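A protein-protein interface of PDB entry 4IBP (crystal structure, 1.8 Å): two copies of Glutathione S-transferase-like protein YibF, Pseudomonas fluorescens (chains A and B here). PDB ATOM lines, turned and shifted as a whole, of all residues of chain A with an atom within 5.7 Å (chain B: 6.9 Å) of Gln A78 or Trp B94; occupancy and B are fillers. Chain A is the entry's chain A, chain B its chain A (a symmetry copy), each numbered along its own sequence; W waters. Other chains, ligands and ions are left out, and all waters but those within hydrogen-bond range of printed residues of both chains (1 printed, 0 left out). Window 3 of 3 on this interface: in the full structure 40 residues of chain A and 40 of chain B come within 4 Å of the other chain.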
ATOM      1  N   GLN A  64      26.829   4.638  27.710  1.00  0.00           N
ATOM      2  CA  GLN A  64      26.708   5.268  26.387  1.00  0.00           C
ATOM      3  C   GLN A  64      28.094   5.535  25.774  1.00  0.00           C
ATOM      4  O   GLN A  64      29.060   5.780  26.503  1.00  0.00           O
ATOM      5  CB  GLN A  64      25.909   6.564  26.502  1.00  0.00           C
ATOM      6  CG  GLN A  64      25.797   7.361  25.212  1.00  0.00           C
ATOM      7  CD  GLN A  64      24.824   8.526  25.324  1.00  0.00           C
ATOM      8  OE1 GLN A  64      23.983   8.569  26.229  1.00  0.00           O
ATOM      9  NE2 GLN A  64      24.934   9.473  24.398  1.00  0.00           N
ATOM     10  N   LEU A  66      30.419   7.768  22.969  1.00  0.00           N
ATOM     11  CA  LEU A  66      30.529   8.911  22.069  1.00  0.00           C
ATOM     12  C   LEU A  66      31.656   8.702  21.055  1.00  0.00           C
ATOM     13  O   LEU A  66      32.725   8.163  21.388  1.00  0.00           O
ATOM     14  CB  LEU A  66      30.792  10.192  22.856  1.00  0.00           C
ATOM     15  CG  LEU A  66      29.841  10.525  23.992  1.00  0.00           C
ATOM     16  CD1 LEU A  66      30.165  11.917  24.551  1.00  0.00           C
ATOM     17  CD2 LEU A  66      28.393  10.468  23.517  1.00  0.00           C
ATOM     18  N   VAL A  71      33.210  15.055  18.359  1.00  0.00           N
ATOM     19  CA  VAL A  71      32.095  14.933  19.299  1.00  0.00           C
ATOM     20  C   VAL A  71      32.622  14.755  20.738  1.00  0.00           C
ATOM     21  O   VAL A  71      32.129  15.374  21.681  1.00  0.00           O
ATOM     22  CB  VAL A  71      31.170  13.755  18.926  1.00  0.00           C
ATOM     23  CG1 VAL A  71      29.994  13.676  19.889  1.00  0.00           C
ATOM     24  CG2 VAL A  71      30.674  13.902  17.491  1.00  0.00           C
ATOM     25  N   LEU A  73      35.555  15.733  21.852  1.00  0.00           N
ATOM     26  CA  LEU A  73      36.179  17.001  22.260  1.00  0.00           C
ATOM     27  C   LEU A  73      35.121  17.998  22.747  1.00  0.00           C
ATOM     28  O   LEU A  73      35.300  18.665  23.761  1.00  0.00           O
ATOM     29  CB  LEU A  73      36.990  17.574  21.108  1.00  0.00           C
ATOM     30  CG  LEU A  73      38.221  16.727  20.777  1.00  0.00           C
ATOM     31  CD1 LEU A  73      38.760  17.094  19.393  1.00  0.00           C
ATOM     32  CD2 LEU A  73      39.321  16.922  21.836  1.00  0.00           C
ATOM     33  N   ASP A  74      33.997  18.067  22.040  1.00  0.00           N
ATOM     34  CA  ASP A  74      32.931  18.988  22.407  1.00  0.00           C
ATOM     35  C   ASP A  74      32.362  18.592  23.769  1.00  0.00           C
ATOM     36  O   ASP A  74      32.162  19.441  24.641  1.00  0.00           O
ATOM     37  CB  ASP A  74      31.819  18.977  21.347  1.00  0.00           C
ATOM     38  CG  ASP A  74      30.749  20.038  21.604  1.00  0.00           C
ATOM     39  OD1 ASP A  74      29.580  19.671  21.808  1.00  0.00           O
ATOM     40  OD2 ASP A  74      31.080  21.236  21.629  1.00  0.00           O
ATOM     41  N   TYR A  75      32.136  17.298  23.959  1.00  0.00           N
ATOM     42  CA  TYR A  75      31.631  16.797  25.242  1.00  0.00           C
ATOM     43  C   TYR A  75      32.564  17.167  26.401  1.00  0.00           C
ATOM     44  O   TYR A  75      32.149  17.746  27.407  1.00  0.00           O
ATOM     45  CB  TYR A  75      31.486  15.284  25.183  1.00  0.00           C
ATOM     46  CG  TYR A  75      31.145  14.664  26.511  1.00  0.00           C
ATOM     47  CD1 TYR A  75      29.854  14.741  27.033  1.00  0.00           C
ATOM     48  CD2 TYR A  75      32.112  13.987  27.235  1.00  0.00           C
ATOM     49  CE1 TYR A  75      29.543  14.159  28.258  1.00  0.00           C
ATOM     50  CE2 TYR A  75      31.817  13.401  28.463  1.00  0.00           C
ATOM     51  CZ  TYR A  75      30.534  13.491  28.965  1.00  0.00           C
ATOM     52  OH  TYR A  75      30.250  12.914  30.181  1.00  0.00           O
ATOM     53  N   LEU A  76      33.829  16.823  26.253  1.00  0.00           N
ATOM     54  CA  LEU A  76      34.777  17.026  27.340  1.00  0.00           C
ATOM     55  C   LEU A  76      35.003  18.505  27.634  1.00  0.00           C
ATOM     56  O   LEU A  76      35.255  18.876  28.788  1.00  0.00           O
ATOM     57  CB  LEU A  76      36.078  16.298  27.051  1.00  0.00           C
ATOM     58  CG  LEU A  76      36.035  14.777  27.037  1.00  0.00           C
ATOM     59  CD1 LEU A  76      37.284  14.248  26.378  1.00  0.00           C
ATOM     60  CD2 LEU A  76      35.870  14.170  28.443  1.00  0.00           C
ATOM     61  N   ASP A  77      34.901  19.354  26.614  1.00  0.00           N
ATOM     62  CA  ASP A  77      35.077  20.791  26.821  1.00  0.00           C
ATOM     63  C   ASP A  77      33.922  21.373  27.644  1.00  0.00           C
ATOM     64  O   ASP A  77      34.067  22.405  28.277  1.00  0.00           O
ATOM     65  CB  ASP A  77      35.211  21.542  25.487  1.00  0.00           C
ATOM     66  CG  ASP A  77      35.627  22.999  25.682  1.00  0.00           C
ATOM     67  OD1 ASP A  77      36.565  23.242  26.473  1.00  0.00           O
ATOM     68  OD2 ASP A  77      35.010  23.896  25.076  1.00  0.00           O
ATOM     69  N   GLN A  78      32.763  20.718  27.627  1.00  0.00           N
ATOM     70  CA  GLN A  78      31.632  21.177  28.418  1.00  0.00           C
ATOM     71  C   GLN A  78      31.630  20.608  29.827  1.00  0.00           C
ATOM     72  O   GLN A  78      30.781  20.967  30.641  1.00  0.00           O
ATOM     73  CB  GLN A  78      30.335  20.756  27.730  1.00  0.00           C
ATOM     74  CG  GLN A  78      30.185  21.362  26.369  1.00  0.00           C
ATOM     75  CD  GLN A  78      29.291  22.565  26.404  1.00  0.00           C
ATOM     76  OE1 GLN A  78      29.524  23.499  27.178  1.00  0.00           O
ATOM     77  NE2 GLN A  78      28.247  22.550  25.581  1.00  0.00           N
ATOM     78  N   GLN A  79      32.576  19.720  30.109  1.00  0.00           N
ATOM     79  CA  GLN A  79      32.614  19.007  31.389  1.00  0.00           C
ATOM     80  C   GLN A  79      33.355  19.745  32.493  1.00  0.00           C
ATOM     81  O   GLN A  79      33.162  19.451  33.674  1.00  0.00           O
ATOM     82  CB  GLN A  79      33.212  17.613  31.201  1.00  0.00           C
ATOM     83  CG  GLN A  79      32.298  16.678  30.425  1.00  0.00           C
ATOM     84  CD  GLN A  79      31.017  16.421  31.176  1.00  0.00           C
ATOM     85  OE1 GLN A  79      31.040  15.876  32.280  1.00  0.00           O
ATOM     86  NE2 GLN A  79      29.900  16.834  30.603  1.00  0.00           N
ATOM     87  N   HIS A  80      34.215  20.685  32.121  1.00  0.00           N
ATOM     88  CA  HIS A  80      34.983  21.432  33.110  1.00  0.00           C
ATOM     89  C   HIS A  80      34.477  22.871  33.205  1.00  0.00           C
ATOM     90  O   HIS A  80      33.772  23.347  32.316  1.00  0.00           O
ATOM     91  CB  HIS A  80      36.457  21.436  32.730  1.00  0.00           C
ATOM     92  CG  HIS A  80      36.734  22.170  31.453  1.00  0.00           C
ATOM     93  ND1 HIS A  80      37.231  23.453  31.440  1.00  0.00           N
ATOM     94  CD2 HIS A  80      36.535  21.816  30.168  1.00  0.00           C
ATOM     95  CE1 HIS A  80      37.339  23.856  30.180  1.00  0.00           C
ATOM     96  NE2 HIS A  80      36.925  22.885  29.391  1.00  0.00           N
ATOM     97  N   PRO B  87      20.824  19.896  19.371  1.00  0.00           N
ATOM     98  CA  PRO B  87      20.541  20.245  20.768  1.00  0.00           C
ATOM     99  C   PRO B  87      21.683  21.072  21.351  1.00  0.00           C
ATOM    100  O   PRO B  87      22.855  20.733  21.159  1.00  0.00           O
ATOM    101  CB  PRO B  87      20.483  18.881  21.464  1.00  0.00           C
ATOM    102  CG  PRO B  87      20.181  17.904  20.374  1.00  0.00           C
ATOM    103  CD  PRO B  87      20.827  18.442  19.137  1.00  0.00           C
ATOM    104  N   ARG B  88      21.365  22.161  22.037  1.00  0.00           N
ATOM    105  CA  ARG B  88      22.438  23.032  22.512  1.00  0.00           C
ATOM    106  C   ARG B  88      23.171  22.465  23.731  1.00  0.00           C
ATOM    107  O   ARG B  88      24.348  22.738  23.925  1.00  0.00           O
ATOM    108  CB  ARG B  88      21.931  24.451  22.760  1.00  0.00           C
ATOM    109  CG  ARG B  88      20.832  24.554  23.792  1.00  0.00           C
ATOM    110  CD  ARG B  88      20.261  25.973  23.858  1.00  0.00           C
ATOM    111  NE  ARG B  88      19.220  26.214  22.856  1.00  0.00           N
ATOM    112  CZ  ARG B  88      17.939  25.885  23.014  1.00  0.00           C
ATOM    113  NH1 ARG B  88      17.539  25.289  24.129  1.00  0.00           N
ATOM    114  NH2 ARG B  88      17.057  26.148  22.059  1.00  0.00           N
ATOM    115  N   ASP B  89      22.478  21.659  24.530  1.00  0.00           N
ATOM    116  CA  ASP B  89      23.079  21.003  25.691  1.00  0.00           C
ATOM    117  C   ASP B  89      22.271  19.774  26.078  1.00  0.00           C
ATOM    118  O   ASP B  89      21.391  19.340  25.332  1.00  0.00           O
ATOM    119  CB  ASP B  89      23.163  21.969  26.876  1.00  0.00           C
ATOM    120  CG  ASP B  89      21.859  22.705  27.119  1.00  0.00           C
ATOM    121  OD1 ASP B  89      20.893  22.065  27.582  1.00  0.00           O
ATOM    122  OD2 ASP B  89      21.798  23.923  26.839  1.00  0.00           O
ATOM    123  N   GLY B  90      22.559  19.210  27.247  1.00  0.00           N
ATOM    124  CA  GLY B  90      21.848  18.022  27.689  1.00  0.00           C
ATOM    125  C   GLY B  90      22.453  16.778  27.066  1.00  0.00           C
ATOM    126  O   GLY B  90      23.295  16.877  26.168  1.00  0.00           O
ATOM    127  N   SER B  91      22.035  15.603  27.530  1.00  0.00           N
ATOM    128  CA  SER B  91      22.603  14.366  27.004  1.00  0.00           C
ATOM    129  C   SER B  91      22.197  14.184  25.547  1.00  0.00           C
ATOM    130  O   SER B  91      22.916  13.561  24.762  1.00  0.00           O
ATOM    131  CB  SER B  91      22.202  13.158  27.849  1.00  0.00           C
ATOM    132  OG  SER B  91      20.809  12.943  27.821  1.00  0.00           O
ATOM    133  N   ALA B  92      21.049  14.756  25.192  1.00  0.00           N
ATOM    134  CA  ALA B  92      20.587  14.752  23.816  1.00  0.00           C
ATOM    135  C   ALA B  92      21.626  15.357  22.867  1.00  0.00           C
ATOM    136  O   ALA B  92      21.758  14.905  21.744  1.00  0.00           O
ATOM    137  CB  ALA B  92      19.249  15.476  23.696  1.00  0.00           C
ATOM    138  N   ARG B  93      22.387  16.357  23.305  1.00  0.00           N
ATOM    139  CA  ARG B  93      23.363  16.939  22.400  1.00  0.00           C
ATOM    140  C   ARG B  93      24.381  15.894  21.951  1.00  0.00           C
ATOM    141  O   ARG B  93      24.606  15.709  20.754  1.00  0.00           O
ATOM    142  CB  ARG B  93      24.097  18.139  23.022  1.00  0.00           C
ATOM    143  CG  ARG B  93      25.169  18.699  22.111  1.00  0.00           C
ATOM    144  CD  ARG B  93      25.831  19.957  22.695  1.00  0.00           C
ATOM    145  NE  ARG B  93      26.923  20.427  21.844  1.00  0.00           N
ATOM    146  CZ  ARG B  93      26.755  21.188  20.770  1.00  0.00           C
ATOM    147  NH1 ARG B  93      25.534  21.566  20.404  1.00  0.00           N
ATOM    148  NH2 ARG B  93      27.805  21.570  20.055  1.00  0.00           N
ATOM    149  N   TRP B  94      24.989  15.184  22.890  1.00  0.00           N
ATOM    150  CA  TRP B  94      26.037  14.274  22.464  1.00  0.00           C
ATOM    151  C   TRP B  94      25.502  12.974  21.896  1.00  0.00           C
ATOM    152  O   TRP B  94      26.177  12.334  21.094  1.00  0.00           O
ATOM    153  CB  TRP B  94      27.115  14.127  23.529  1.00  0.00           C
ATOM    154  CG  TRP B  94      27.706  15.498  23.758  1.00  0.00           C
ATOM    155  CD1 TRP B  94      28.589  16.165  22.952  1.00  0.00           C
ATOM    156  CD2 TRP B  94      27.379  16.387  24.815  1.00  0.00           C
ATOM    157  NE1 TRP B  94      28.853  17.421  23.466  1.00  0.00           N
ATOM    158  CE2 TRP B  94      28.125  17.573  24.623  1.00  0.00           C
ATOM    159  CE3 TRP B  94      26.535  16.293  25.928  1.00  0.00           C
ATOM    160  CZ2 TRP B  94      28.047  18.655  25.496  1.00  0.00           C
ATOM    161  CZ3 TRP B  94      26.461  17.362  26.795  1.00  0.00           C
ATOM    162  CH2 TRP B  94      27.216  18.527  26.580  1.00  0.00           C
ATOM    163  N   ARG B  95      24.275  12.623  22.261  1.00  0.00           N
ATOM    164  CA  ARG B  95      23.642  11.464  21.649  1.00  0.00           C
ATOM    165  C   ARG B  95      23.356  11.731  20.164  1.00  0.00           C
ATOM    166  O   ARG B  95      23.723  10.919  19.292  1.00  0.00           O
ATOM    167  CB  ARG B  95      22.351  11.088  22.385  1.00  0.00           C
ATOM    168  CG  ARG B  95      21.612   9.924  21.759  1.00  0.00           C
ATOM    169  CD  ARG B  95      22.507   8.707  21.577  1.00  0.00           C
ATOM    170  NE  ARG B  95      21.740   7.541  21.116  1.00  0.00           N
ATOM    171  CZ  ARG B  95      22.290   6.439  20.617  1.00  0.00           C
ATOM    172  NH1 ARG B  95      23.604   6.348  20.520  1.00  0.00           N
ATOM    173  NH2 ARG B  95      21.524   5.429  20.211  1.00  0.00           N
ATOM    174  N   ARG B  96      22.711  12.862  19.874  1.00  0.00           N
ATOM    175  CA  ARG B  96      22.346  13.189  18.492  1.00  0.00           C
ATOM    176  C   ARG B  96      23.596  13.490  17.685  1.00  0.00           C
ATOM    177  O   ARG B  96      23.670  13.174  16.517  1.00  0.00           O
ATOM    178  CB  ARG B  96      21.397  14.395  18.392  1.00  0.00           C
ATOM    179  CG  ARG B  96      20.199  14.426  19.343  1.00  0.00           C
ATOM    180  CD  ARG B  96      19.266  13.259  19.180  1.00  0.00           C
ATOM    181  NE  ARG B  96      18.602  13.228  17.880  1.00  0.00           N
ATOM    182  CZ  ARG B  96      17.426  12.639  17.680  1.00  0.00           C
ATOM    183  NH1 ARG B  96      16.811  12.068  18.706  1.00  0.00           N
ATOM    184  NH2 ARG B  96      16.860  12.621  16.474  1.00  0.00           N
ATOM    185  N   LEU B  97      24.601  14.110  18.296  1.00  0.00           N
ATOM    186  CA  LEU B  97      25.819  14.376  17.532  1.00  0.00           C
ATOM    187  C   LEU B  97      26.584  13.079  17.213  1.00  0.00           C
ATOM    188  O   LEU B  97      27.245  12.967  16.178  1.00  0.00           O
ATOM    189  CB  LEU B  97      26.726  15.378  18.285  1.00  0.00           C
ATOM    190  CG  LEU B  97      26.239  16.830  18.161  1.00  0.00           C
ATOM    191  CD1 LEU B  97      27.223  17.815  18.817  1.00  0.00           C
ATOM    192  CD2 LEU B  97      26.028  17.206  16.701  1.00  0.00           C
ATOM    193  N   THR B  98      26.477  12.089  18.091  1.00  0.00           N
ATOM    194  CA  THR B  98      27.141  10.804  17.858  1.00  0.00           C
ATOM    195  C   THR B  98      26.432  10.040  16.729  1.00  0.00           C
ATOM    196  O   THR B  98      27.084   9.436  15.865  1.00  0.00           O
ATOM    197  CB  THR B  98      27.201   9.936  19.137  1.00  0.00           C
ATOM    198  OG1 THR B  98      28.096  10.530  20.093  1.00  0.00           O
ATOM    199  CG2 THR B  98      27.706   8.523  18.813  1.00  0.00           C
ATOM    200  N   LEU B  99      25.110  10.057  16.750  1.00  0.00           N
ATOM    201  CA  LEU B  99      24.333   9.458  15.673  1.00  0.00           C
ATOM    202  C   LEU B  99      24.673  10.115  14.331  1.00  0.00           C
ATOM    203  O   LEU B  99      24.830   9.436  13.315  1.00  0.00           O
ATOM    204  CB  LEU B  99      22.838   9.599  15.955  1.00  0.00           C
ATOM    205  CG  LEU B  99      22.297   8.710  17.069  1.00  0.00           C
ATOM    206  CD1 LEU B  99      20.809   8.913  17.227  1.00  0.00           C
ATOM    207  CD2 LEU B  99      22.596   7.243  16.767  1.00  0.00           C
HETATM  208  O   HOH W   1      24.872  11.937  25.715  1.00  0.00           O
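The side-chain carboxylate (OD1) of Asp A74 is in salt-bridge range of the guanidinium group (NE) of Arg B93, at 2.8 Å. OD1 of Asp A74 sits at hydrogen-bond distance from NE1 of Trp B94 (2.9 Å). N of Tyr A75 lies close to NE1 of Trp B94 (3.3 Å).
The backbone carbonyl oxygen (O) of Pro B87 lies within hydrogen-bond range of the guanidinium group (NH1) of Arg B93 (2.9 Å). The backbone carbonyl oxygen (O) of Trp B94 is in hydrogen-bond range of the side-chain hydroxyl (OG1) of Thr B98, at 2.8 Å.
Among the printed residues, pairs that only touch across the chains: Leu A66 with Thr B98, Gln A78 with Trp B94, Gln A64 with Arg B95, Val A71 with Thr B98, Leu A66 with Trp B94, Val A71 with Leu B97 and Val A71 with Trp B94.
Of chain A, only Leu A66, Val A71, Asp A74, Tyr A75 and Gln A78 come within 4 Å of Trp B94. Of the printed residues of chain B, Asp A74 touches Arg B93 (2.8 Å) and Trp B94 (2.9 Å). Of the printed residues of chain B, Leu A66 touches Trp B94 and Thr B98. Of the printed residues of chain B, Val A71 touches Trp B94, Leu B97 and Thr B98. Gly B90 touches none of the printed residues of chain A. Ser B91 touches none of the printed residues of chain A.
Of the 11 printed residues of chain A, 6 touch a printed residue of chain B. Hydrophobic or aromatic side chains of chain A within 4 Å of the printed part of chain B: Leu A66, Val A71 and Tyr A75. Among the printed residues, 10 pairs touch across the chains.
No position is printed for both chains. Of the 10 pairs that touch across the chains among the printed residues, none has its exchanged pair printed and touching as well.
Water W1 lies within hydrogen-bond range of the backbone carbonyl oxygen (O) of Ser B91 (2.7 Å) and the side-chain amide nitrogen (NE2) of Gln A64 (2.8 Å).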
